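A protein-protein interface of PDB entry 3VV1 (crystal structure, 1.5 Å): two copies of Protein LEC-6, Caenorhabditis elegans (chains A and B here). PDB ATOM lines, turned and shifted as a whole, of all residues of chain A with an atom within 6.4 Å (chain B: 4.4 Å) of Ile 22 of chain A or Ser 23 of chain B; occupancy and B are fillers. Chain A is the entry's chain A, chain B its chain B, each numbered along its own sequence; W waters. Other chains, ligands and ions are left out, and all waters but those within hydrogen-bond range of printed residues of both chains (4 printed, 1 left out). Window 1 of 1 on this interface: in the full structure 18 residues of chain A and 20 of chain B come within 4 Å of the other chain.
The backbone carbonyl oxygen (O) of Gly 21 of chain A lies within hydrogen-bond range of the backbone NH (N) of Ser 23 of chain B (3.0 Å).
The backbone NH of Ile 22 of chain A is in hydrogen-bond range of the backbone carbonyl oxygen of Pro 38 of chain B, 3.1 Å away.
O of Ile 22 of chain A lies within hydrogen-bond range of N of Gln 40 of chain B (3.0 Å).
O of Gln 40 of chain B lies within hydrogen-bond range of N of Phe 24 of chain A, at 3.1 Å.
The side-chain amide nitrogen (ND2) of Asn 26 of chain A is in hydrogen-bond range of the backbone carbonyl oxygen (O) of Phe 24 of chain B, 3.3 Å away.
The backbone carbonyl oxygen (O) of Pro 38 of chain A lies within hydrogen-bond range of the backbone NH (N) of Phe 24 of chain B, at 2.8 Å.
Hydrophobic or aromatic side chains of chain A that line the printed part of chain B: Ile 20, Ile 22, Phe 24, Phe 28, Ile 37 and Pro 38.
Along chain A the printed residues that touch a printed residue of chain B span positions 20 to 39.
Hydrophobic or aromatic side chains of chain B within 4 Å of the printed part of chain A: Ile 22, Phe 24, Phe 28, Ile 37, Pro 38, Val 39 and Val 158.
Among the printed residues, 31 pairs touch across the chains.
Among the printed residues, merely in contact across the chains: Ile 20 of chain A with Ser 23 of chain B (3.4 Å), Ile 20 of chain A with Pro 38 of chain B (3.7 Å), Gly 21 of chain A with Ile 22 of chain B (3.4 Å), Gly 21 of chain A with Pro 38 of chain B (3.4 Å), Ile 22 of chain A with Ser 23 of chain B (3.8 Å), Ile 22 of chain A with Arg 25 of chain B (3.4 Å), Ile 22 of chain A with Phe 28 of chain B (3.9 Å), Ile 22 of chain A with Ile 37 of chain B (3.6 Å), Ile 22 of chain A with Val 39 of chain B (3.2 Å), Ile 22 of chain A with Val 158 of chain B (3.7 Å), Ser 23 of chain A with Gln 40 of chain B (3.4 Å), Ser 23 of chain A with Val 158 of chain B (3.6 Å), Phe 24 of chain A with Val 39 of chain B (3.8 Å), Phe 24 of chain A with Val 158 of chain B (3.6 Å), Phe 28 of chain A with Ile 22 of chain B (3.5 Å), Phe 28 of chain A with Ser 23 of chain B (3.2 Å), Phe 28 of chain A with Phe 24 of chain B (3.7 Å), Phe 28 of chain A with Gln 40 of chain B (3.6 Å), Ile 37 of chain A with Ile 22 of chain B (3.6 Å), Ile 37 of chain A with Ser 23 of chain B (3.7 Å), Ile 37 of chain A with Phe 24 of chain B (3.4 Å), Pro 38 of chain A with Ile 22 of chain B (3.4 Å), Pro 38 of chain A with Ser 23 of chain B (3.6 Å), Pro 38 of chain A with Arg 25 of chain B (3.8 Å) and Val 39 of chain A with Arg 25 of chain B (3.8 Å).
Of chain B, only Ser 23 (3.8 Å), Arg 25 (3.4 Å), Phe 28 (3.9 Å), Ile 37 (3.6 Å), Pro 38 (3.1 Å), Val 39 (3.2 Å), Gln 40 (3.0 Å) and Val 158 (3.7 Å) come within 4 Å of Ile 22 of chain A.
Of the printed residues of chain B, Ile 37 of chain A touches Ile 22 (3.6 Å), Ser 23 (3.7 Å) and Phe 24 (3.4 Å).
Of the printed residues of chain B, Val 39 of chain A touches Arg 25 (3.8 Å).
The nearest residue of chain A that does not touch Ser 23 of chain B is Asn 26 of chain A (4.2 Å).
Water W4 lies within hydrogen-bond range of O of Ile 20 of chain A (2.6 Å) and O of Pro 38 of chain B (3.0 Å).
Water W3 bridges the side-chain hydroxyl (OG) of Ser 23 of chain A (2.6 Å) and the side-chain amide nitrogen (NE2) of Gln 40 of chain B (3.2 Å).
Water W1 lies within hydrogen-bond range of OD1 of Asn 26 of chain A (2.7 Å), O of Ser 23 of chain B (2.8 Å) and N of Ser 23 of chain A (2.9 Å).
Water W2 bridges the side-chain amide oxygen (OE1) of Gln 40 of chain B and the backbone carbonyl oxygen (O) of Ile 22 of chain A.
OG of Ser 23 of chain A is in hydrogen-bond range of N of Asn 26 of chain A (3.2 Å).
OG of Ser 23 of chain B lies within hydrogen-bond range of N of Arg 25 of chain B (2.9 Å).
Ile 22 of chain A touches Phe 28 of chain B, and with the chains exchanged Phe 28 of chain A touches Ile 22 of chain B.
Ile 22 of chain A touches Val 39 of chain B, but with the chains exchanged Val 39 of chain A does not touch Ile 22 of chain B (7.3 Å).
Phe 28 of chain A touches Ser 23 of chain B, but with the chains exchanged Ser 23 of chain A does not touch Phe 28 of chain B (8.8 Å).
Ile 37 of chain A touches Phe 24 of chain B, but with the chains exchanged Phe 24 of chain A does not touch Ile 37 of chain B (7.4 Å).
Positions printed for both chains: 22, 23, 24, 28, 37, 38 and 39.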
ATOM      1  N   ILE A  20       7.947  -2.678  31.165  1.00  0.00           N
ATOM      2  CA  ILE A  20       8.074  -2.075  29.782  1.00  0.00           C
ATOM      3  C   ILE A  20       8.694  -3.128  28.868  1.00  0.00           C
ATOM      4  O   ILE A  20       9.842  -3.544  29.084  1.00  0.00           O
ATOM      5  CB  ILE A  20       8.999  -0.851  29.716  1.00  0.00           C
ATOM      6  CG1 ILE A  20       8.516   0.260  30.682  1.00  0.00           C
ATOM      7  CG2 ILE A  20       9.055  -0.372  28.277  1.00  0.00           C
ATOM      8  CD1 ILE A  20       9.286   1.562  30.629  1.00  0.00           C
ATOM      9  N   GLY A  21       7.935  -3.543  27.864  1.00  0.00           N
ATOM     10  CA  GLY A  21       8.357  -4.599  26.955  1.00  0.00           C
ATOM     11  C   GLY A  21       8.980  -4.051  25.686  1.00  0.00           C
ATOM     12  O   GLY A  21       8.534  -3.046  25.121  1.00  0.00           O
ATOM     13  N   ILE A  22       9.967  -4.795  25.189  1.00  0.00           N
ATOM     14  CA  ILE A  22      10.615  -4.448  23.919  1.00  0.00           C
ATOM     15  C   ILE A  22      10.427  -5.643  22.983  1.00  0.00           C
ATOM     16  O   ILE A  22       9.959  -6.726  23.385  1.00  0.00           O
ATOM     17  CB  ILE A  22      12.139  -4.123  24.132  1.00  0.00           C
ATOM     18  CG1 ILE A  22      12.886  -5.315  24.773  1.00  0.00           C
ATOM     19  CG2 ILE A  22      12.314  -2.817  24.925  1.00  0.00           C
ATOM     20  CD1 ILE A  22      14.383  -5.053  25.077  1.00  0.00           C
ATOM     21  N   SER A  23      10.705  -5.400  21.711  1.00  0.00           N
ATOM     22  CA  SER A  23      10.507  -6.391  20.671  1.00  0.00           C
ATOM     23  C   SER A  23      11.757  -6.619  19.828  1.00  0.00           C
ATOM     24  O   SER A  23      12.403  -5.647  19.435  1.00  0.00           O
ATOM     25  CB  SER A  23       9.398  -5.829  19.785  1.00  0.00           C
ATOM     26  OG  SER A  23       9.281  -6.578  18.549  1.00  0.00           O
ATOM     27  N   PHE A  24      12.012  -7.881  19.495  1.00  0.00           N
ATOM     28  CA  PHE A  24      13.157  -8.244  18.629  1.00  0.00           C
ATOM     29  C   PHE A  24      12.959  -7.694  17.222  1.00  0.00           C
ATOM     30  O   PHE A  24      13.948  -7.571  16.494  1.00  0.00           O
ATOM     31  CB  PHE A  24      13.339  -9.750  18.574  1.00  0.00           C
ATOM     32  CG  PHE A  24      13.905 -10.307  19.833  1.00  0.00           C
ATOM     33  CD1 PHE A  24      13.071 -10.662  20.871  1.00  0.00           C
ATOM     34  CD2 PHE A  24      15.298 -10.516  19.977  1.00  0.00           C
ATOM     35  CE1 PHE A  24      13.631 -11.175  22.049  1.00  0.00           C
ATOM     36  CE2 PHE A  24      15.845 -11.003  21.147  1.00  0.00           C
ATOM     37  CZ  PHE A  24      15.018 -11.405  22.190  1.00  0.00           C
ATOM     38  N   ASN A  26      11.205  -4.659  16.904  1.00  0.00           N
ATOM     39  CA  ASN A  26      10.861  -3.231  17.151  1.00  0.00           C
ATOM     40  C   ASN A  26       9.490  -2.854  16.592  1.00  0.00           C
ATOM     41  O   ASN A  26       9.298  -1.780  16.014  1.00  0.00           O
ATOM     42  CB  ASN A  26      11.983  -2.259  16.679  1.00  0.00           C
ATOM     43  CG  ASN A  26      12.372  -1.276  17.771  1.00  0.00           C
ATOM     44  OD1 ASN A  26      12.017  -1.493  18.903  1.00  0.00           O
ATOM     45  ND2 ASN A  26      13.087  -0.203  17.441  1.00  0.00           N
ATOM     46  N   PHE A  28       5.073  -3.297  17.308  1.00  0.00           N
ATOM     47  CA  PHE A  28       3.979  -3.643  18.245  1.00  0.00           C
ATOM     48  C   PHE A  28       2.639  -3.561  17.543  1.00  0.00           C
ATOM     49  O   PHE A  28       2.446  -2.739  16.648  1.00  0.00           O
ATOM     50  CB  PHE A  28       4.014  -2.694  19.444  1.00  0.00           C
ATOM     51  CG  PHE A  28       5.325  -2.750  20.174  1.00  0.00           C
ATOM     52  CD1 PHE A  28       5.579  -3.768  21.136  1.00  0.00           C
ATOM     53  CD2 PHE A  28       6.327  -1.777  19.921  1.00  0.00           C
ATOM     54  CE1 PHE A  28       6.797  -3.811  21.841  1.00  0.00           C
ATOM     55  CE2 PHE A  28       7.550  -1.843  20.658  1.00  0.00           C
ATOM     56  CZ  PHE A  28       7.779  -2.886  21.573  1.00  0.00           C
ATOM     57  N   ILE A  37       5.135   5.879  23.391  1.00  0.00           N
ATOM     58  CA  ILE A  37       6.143   4.822  23.230  1.00  0.00           C
ATOM     59  C   ILE A  37       7.550   5.426  23.222  1.00  0.00           C
ATOM     60  O   ILE A  37       7.859   6.228  22.323  1.00  0.00           O
ATOM     61  CB  ILE A  37       5.971   4.035  21.911  1.00  0.00           C
ATOM     62  CG1 ILE A  37       4.494   3.618  21.687  1.00  0.00           C
ATOM     63  CG2 ILE A  37       6.836   2.768  21.958  1.00  0.00           C
ATOM     64  CD1 ILE A  37       4.231   2.972  20.340  1.00  0.00           C
ATOM     65  N   PRO A  38       8.375   5.055  24.225  1.00  0.00           N
ATOM     66  CA  PRO A  38       9.756   5.579  24.247  1.00  0.00           C
ATOM     67  C   PRO A  38      10.535   5.185  22.990  1.00  0.00           C
ATOM     68  O   PRO A  38      10.310   4.099  22.441  1.00  0.00           O
ATOM     69  CB  PRO A  38      10.356   4.870  25.433  1.00  0.00           C
ATOM     70  CG  PRO A  38       9.199   4.669  26.408  1.00  0.00           C
ATOM     71  CD  PRO A  38       8.030   4.346  25.493  1.00  0.00           C
ATOM     72  N   VAL A  39      11.492   6.012  22.599  1.00  0.00           N
ATOM     73  CA  VAL A  39      12.358   5.707  21.446  1.00  0.00           C
ATOM     74  C   VAL A  39      13.681   6.408  21.688  1.00  0.00           C
ATOM     75  O   VAL A  39      13.715   7.486  22.303  1.00  0.00           O
ATOM     76  CB  VAL A  39      11.684   6.155  20.120  1.00  0.00           C
ATOM     77  CG1 VAL A  39      11.479   7.679  20.080  1.00  0.00           C
ATOM     78  CG2 VAL A  39      12.496   5.672  18.878  1.00  0.00           C
ATOM     79  N   ILE B  22       4.974  -0.599  26.405  1.00  0.00           N
ATOM     80  CA  ILE B  22       5.832  -0.997  25.292  1.00  0.00           C
ATOM     81  C   ILE B  22       6.864   0.109  24.958  1.00  0.00           C
ATOM     82  O   ILE B  22       6.656   1.283  25.222  1.00  0.00           O
ATOM     83  CB  ILE B  22       5.010  -1.281  24.012  1.00  0.00           C
ATOM     84  CG1 ILE B  22       4.119  -0.094  23.646  1.00  0.00           C
ATOM     85  CG2 ILE B  22       4.215  -2.604  24.156  1.00  0.00           C
ATOM     86  CD1 ILE B  22       3.546  -0.127  22.230  1.00  0.00           C
ATOM     87  N   SER B  23       7.947  -0.271  24.295  1.00  0.00           N
ATOM     88  CA  SER B  23       9.054   0.654  24.039  1.00  0.00           C
ATOM     89  C   SER B  23       9.844   0.294  22.803  1.00  0.00           C
ATOM     90  O   SER B  23      10.079  -0.898  22.582  1.00  0.00           O
ATOM     91  CB  SER B  23      10.057   0.535  25.194  1.00  0.00           C
ATOM     92  OG  SER B  23      11.140   1.403  24.935  1.00  0.00           O
ATOM     93  N   PHE B  24      10.223   1.300  22.049  1.00  0.00           N
ATOM     94  CA  PHE B  24      11.091   1.076  20.914  1.00  0.00           C
ATOM     95  C   PHE B  24      12.563   1.145  21.289  1.00  0.00           C
ATOM     96  O   PHE B  24      13.445   1.125  20.395  1.00  0.00           O
ATOM     97  CB  PHE B  24      10.854   2.127  19.840  1.00  0.00           C
ATOM     98  CG  PHE B  24       9.539   2.002  19.143  1.00  0.00           C
ATOM     99  CD1 PHE B  24       9.190   0.815  18.529  1.00  0.00           C
ATOM    100  CD2 PHE B  24       8.690   3.102  19.068  1.00  0.00           C
ATOM    101  CE1 PHE B  24       7.968   0.739  17.845  1.00  0.00           C
ATOM    102  CE2 PHE B  24       7.472   3.050  18.366  1.00  0.00           C
ATOM    103  CZ  PHE B  24       7.138   1.843  17.768  1.00  0.00           C
ATOM    104  N   ARG B  25      12.856   1.231  22.605  1.00  0.00           N
ATOM    105  CA  ARG B  25      14.282   1.269  23.043  1.00  0.00           C
ATOM    106  C   ARG B  25      14.818  -0.161  23.141  1.00  0.00           C
ATOM    107  O   ARG B  25      14.938  -0.762  24.234  1.00  0.00           O
ATOM    108  CB  ARG B  25      14.417   2.038  24.366  1.00  0.00           C
ATOM    109  CG  ARG B  25      14.101   3.529  24.208  1.00  0.00           C
ATOM    110  CD  ARG B  25      14.258   4.310  25.506  1.00  0.00           C
ATOM    111  NE  ARG B  25      15.681   4.290  25.848  1.00  0.00           N
ATOM    112  CZ  ARG B  25      16.230   4.505  27.032  1.00  0.00           C
ATOM    113  NH1 ARG B  25      15.506   4.917  28.091  1.00  0.00           N
ATOM    114  NH2 ARG B  25      17.565   4.385  27.127  1.00  0.00           N
ATOM    115  N   PHE B  28      19.734  -0.805  25.386  1.00  0.00           N
ATOM    116  CA  PHE B  28      19.836   0.012  26.598  1.00  0.00           C
ATOM    117  C   PHE B  28      21.126  -0.328  27.305  1.00  0.00           C
ATOM    118  O   PHE B  28      21.735  -1.409  27.061  1.00  0.00           O
ATOM    119  CB  PHE B  28      18.560  -0.115  27.474  1.00  0.00           C
ATOM    120  CG  PHE B  28      18.220  -1.527  27.914  1.00  0.00           C
ATOM    121  CD1 PHE B  28      17.485  -2.391  27.079  1.00  0.00           C
ATOM    122  CD2 PHE B  28      18.675  -2.004  29.138  1.00  0.00           C
ATOM    123  CE1 PHE B  28      17.178  -3.716  27.504  1.00  0.00           C
ATOM    124  CE2 PHE B  28      18.372  -3.302  29.565  1.00  0.00           C
ATOM    125  CZ  PHE B  28      17.662  -4.161  28.737  1.00  0.00           C
ATOM    126  N   ILE B  37      14.032  -8.406  31.597  1.00  0.00           N
ATOM    127  CA  ILE B  37      13.770  -7.750  30.316  1.00  0.00           C
ATOM    128  C   ILE B  37      12.508  -8.414  29.721  1.00  0.00           C
ATOM    129  O   ILE B  37      12.612  -9.522  29.174  1.00  0.00           O
ATOM    130  CB  ILE B  37      14.912  -7.913  29.291  1.00  0.00           C
ATOM    131  CG1 ILE B  37      16.323  -7.623  29.898  1.00  0.00           C
ATOM    132  CG2 ILE B  37      14.596  -6.979  28.065  1.00  0.00           C
ATOM    133  CD1 ILE B  37      17.466  -7.891  28.932  1.00  0.00           C
ATOM    134  N   PRO B  38      11.327  -7.787  29.840  1.00  0.00           N
ATOM    135  CA  PRO B  38      10.106  -8.278  29.126  1.00  0.00           C
ATOM    136  C   PRO B  38      10.332  -8.074  27.623  1.00  0.00           C
ATOM    137  O   PRO B  38      10.737  -6.982  27.188  1.00  0.00           O
ATOM    138  CB  PRO B  38       8.994  -7.404  29.643  1.00  0.00           C
ATOM    139  CG  PRO B  38       9.525  -6.757  30.871  1.00  0.00           C
ATOM    140  CD  PRO B  38      11.020  -6.659  30.720  1.00  0.00           C
ATOM    141  N   VAL B  39      10.091  -9.147  26.891  1.00  0.00           N
ATOM    142  CA  VAL B  39      10.297  -9.186  25.424  1.00  0.00           C
ATOM    143  C   VAL B  39       9.152  -9.828  24.658  1.00  0.00           C
ATOM    144  O   VAL B  39       8.325 -10.539  25.254  1.00  0.00           O
ATOM    145  CB  VAL B  39      11.618  -9.904  25.045  1.00  0.00           C
ATOM    146  CG1 VAL B  39      12.823  -9.233  25.712  1.00  0.00           C
ATOM    147  CG2 VAL B  39      11.567 -11.394  25.437  1.00  0.00           C
ATOM    148  N   GLN B  40       9.123  -9.564  23.344  1.00  0.00           N
ATOM    149  CA  GLN B  40       8.284 -10.319  22.432  1.00  0.00           C
ATOM    150  C   GLN B  40       9.019 -10.443  21.114  1.00  0.00           C
ATOM    151  O   GLN B  40       9.969  -9.707  20.840  1.00  0.00           O
ATOM    152  CB  GLN B  40       6.932  -9.611  22.188  1.00  0.00           C
ATOM    153  CG  GLN B  40       7.045  -8.184  21.681  1.00  0.00           C
ATOM    154  CD  GLN B  40       5.727  -7.464  21.768  1.00  0.00           C
ATOM    155  OE1 GLN B  40       5.288  -6.967  22.839  1.00  0.00           O
ATOM    156  NE2 GLN B  40       5.076  -7.389  20.633  1.00  0.00           N
ATOM    157  N   VAL B 158      18.193  -6.103  21.510  1.00  0.00           N
ATOM    158  CA  VAL B 158      17.403  -7.119  20.844  1.00  0.00           C
ATOM    159  C   VAL B 158      17.161  -6.680  19.396  1.00  0.00           C
ATOM    160  O   VAL B 158      16.871  -5.492  19.109  1.00  0.00           O
ATOM    161  CB  VAL B 158      16.077  -7.437  21.638  1.00  0.00           C
ATOM    162  CG1 VAL B 158      16.356  -7.914  23.067  1.00  0.00           C
ATOM    163  CG2 VAL B 158      15.148  -6.237  21.662  1.00  0.00           C
HETATM  164  O   HOH W   1      11.645  -2.738  21.233  1.00  0.00           O
HETATM  165  O   HOH W   2       7.378  -6.825  24.766  1.00  0.00           O
HETATM  166  O   HOH W   3       7.029  -7.825  18.148  1.00  0.00           O
HETATM  167  O   HOH W   4      12.073  -4.549  28.316  1.00  0.00           O
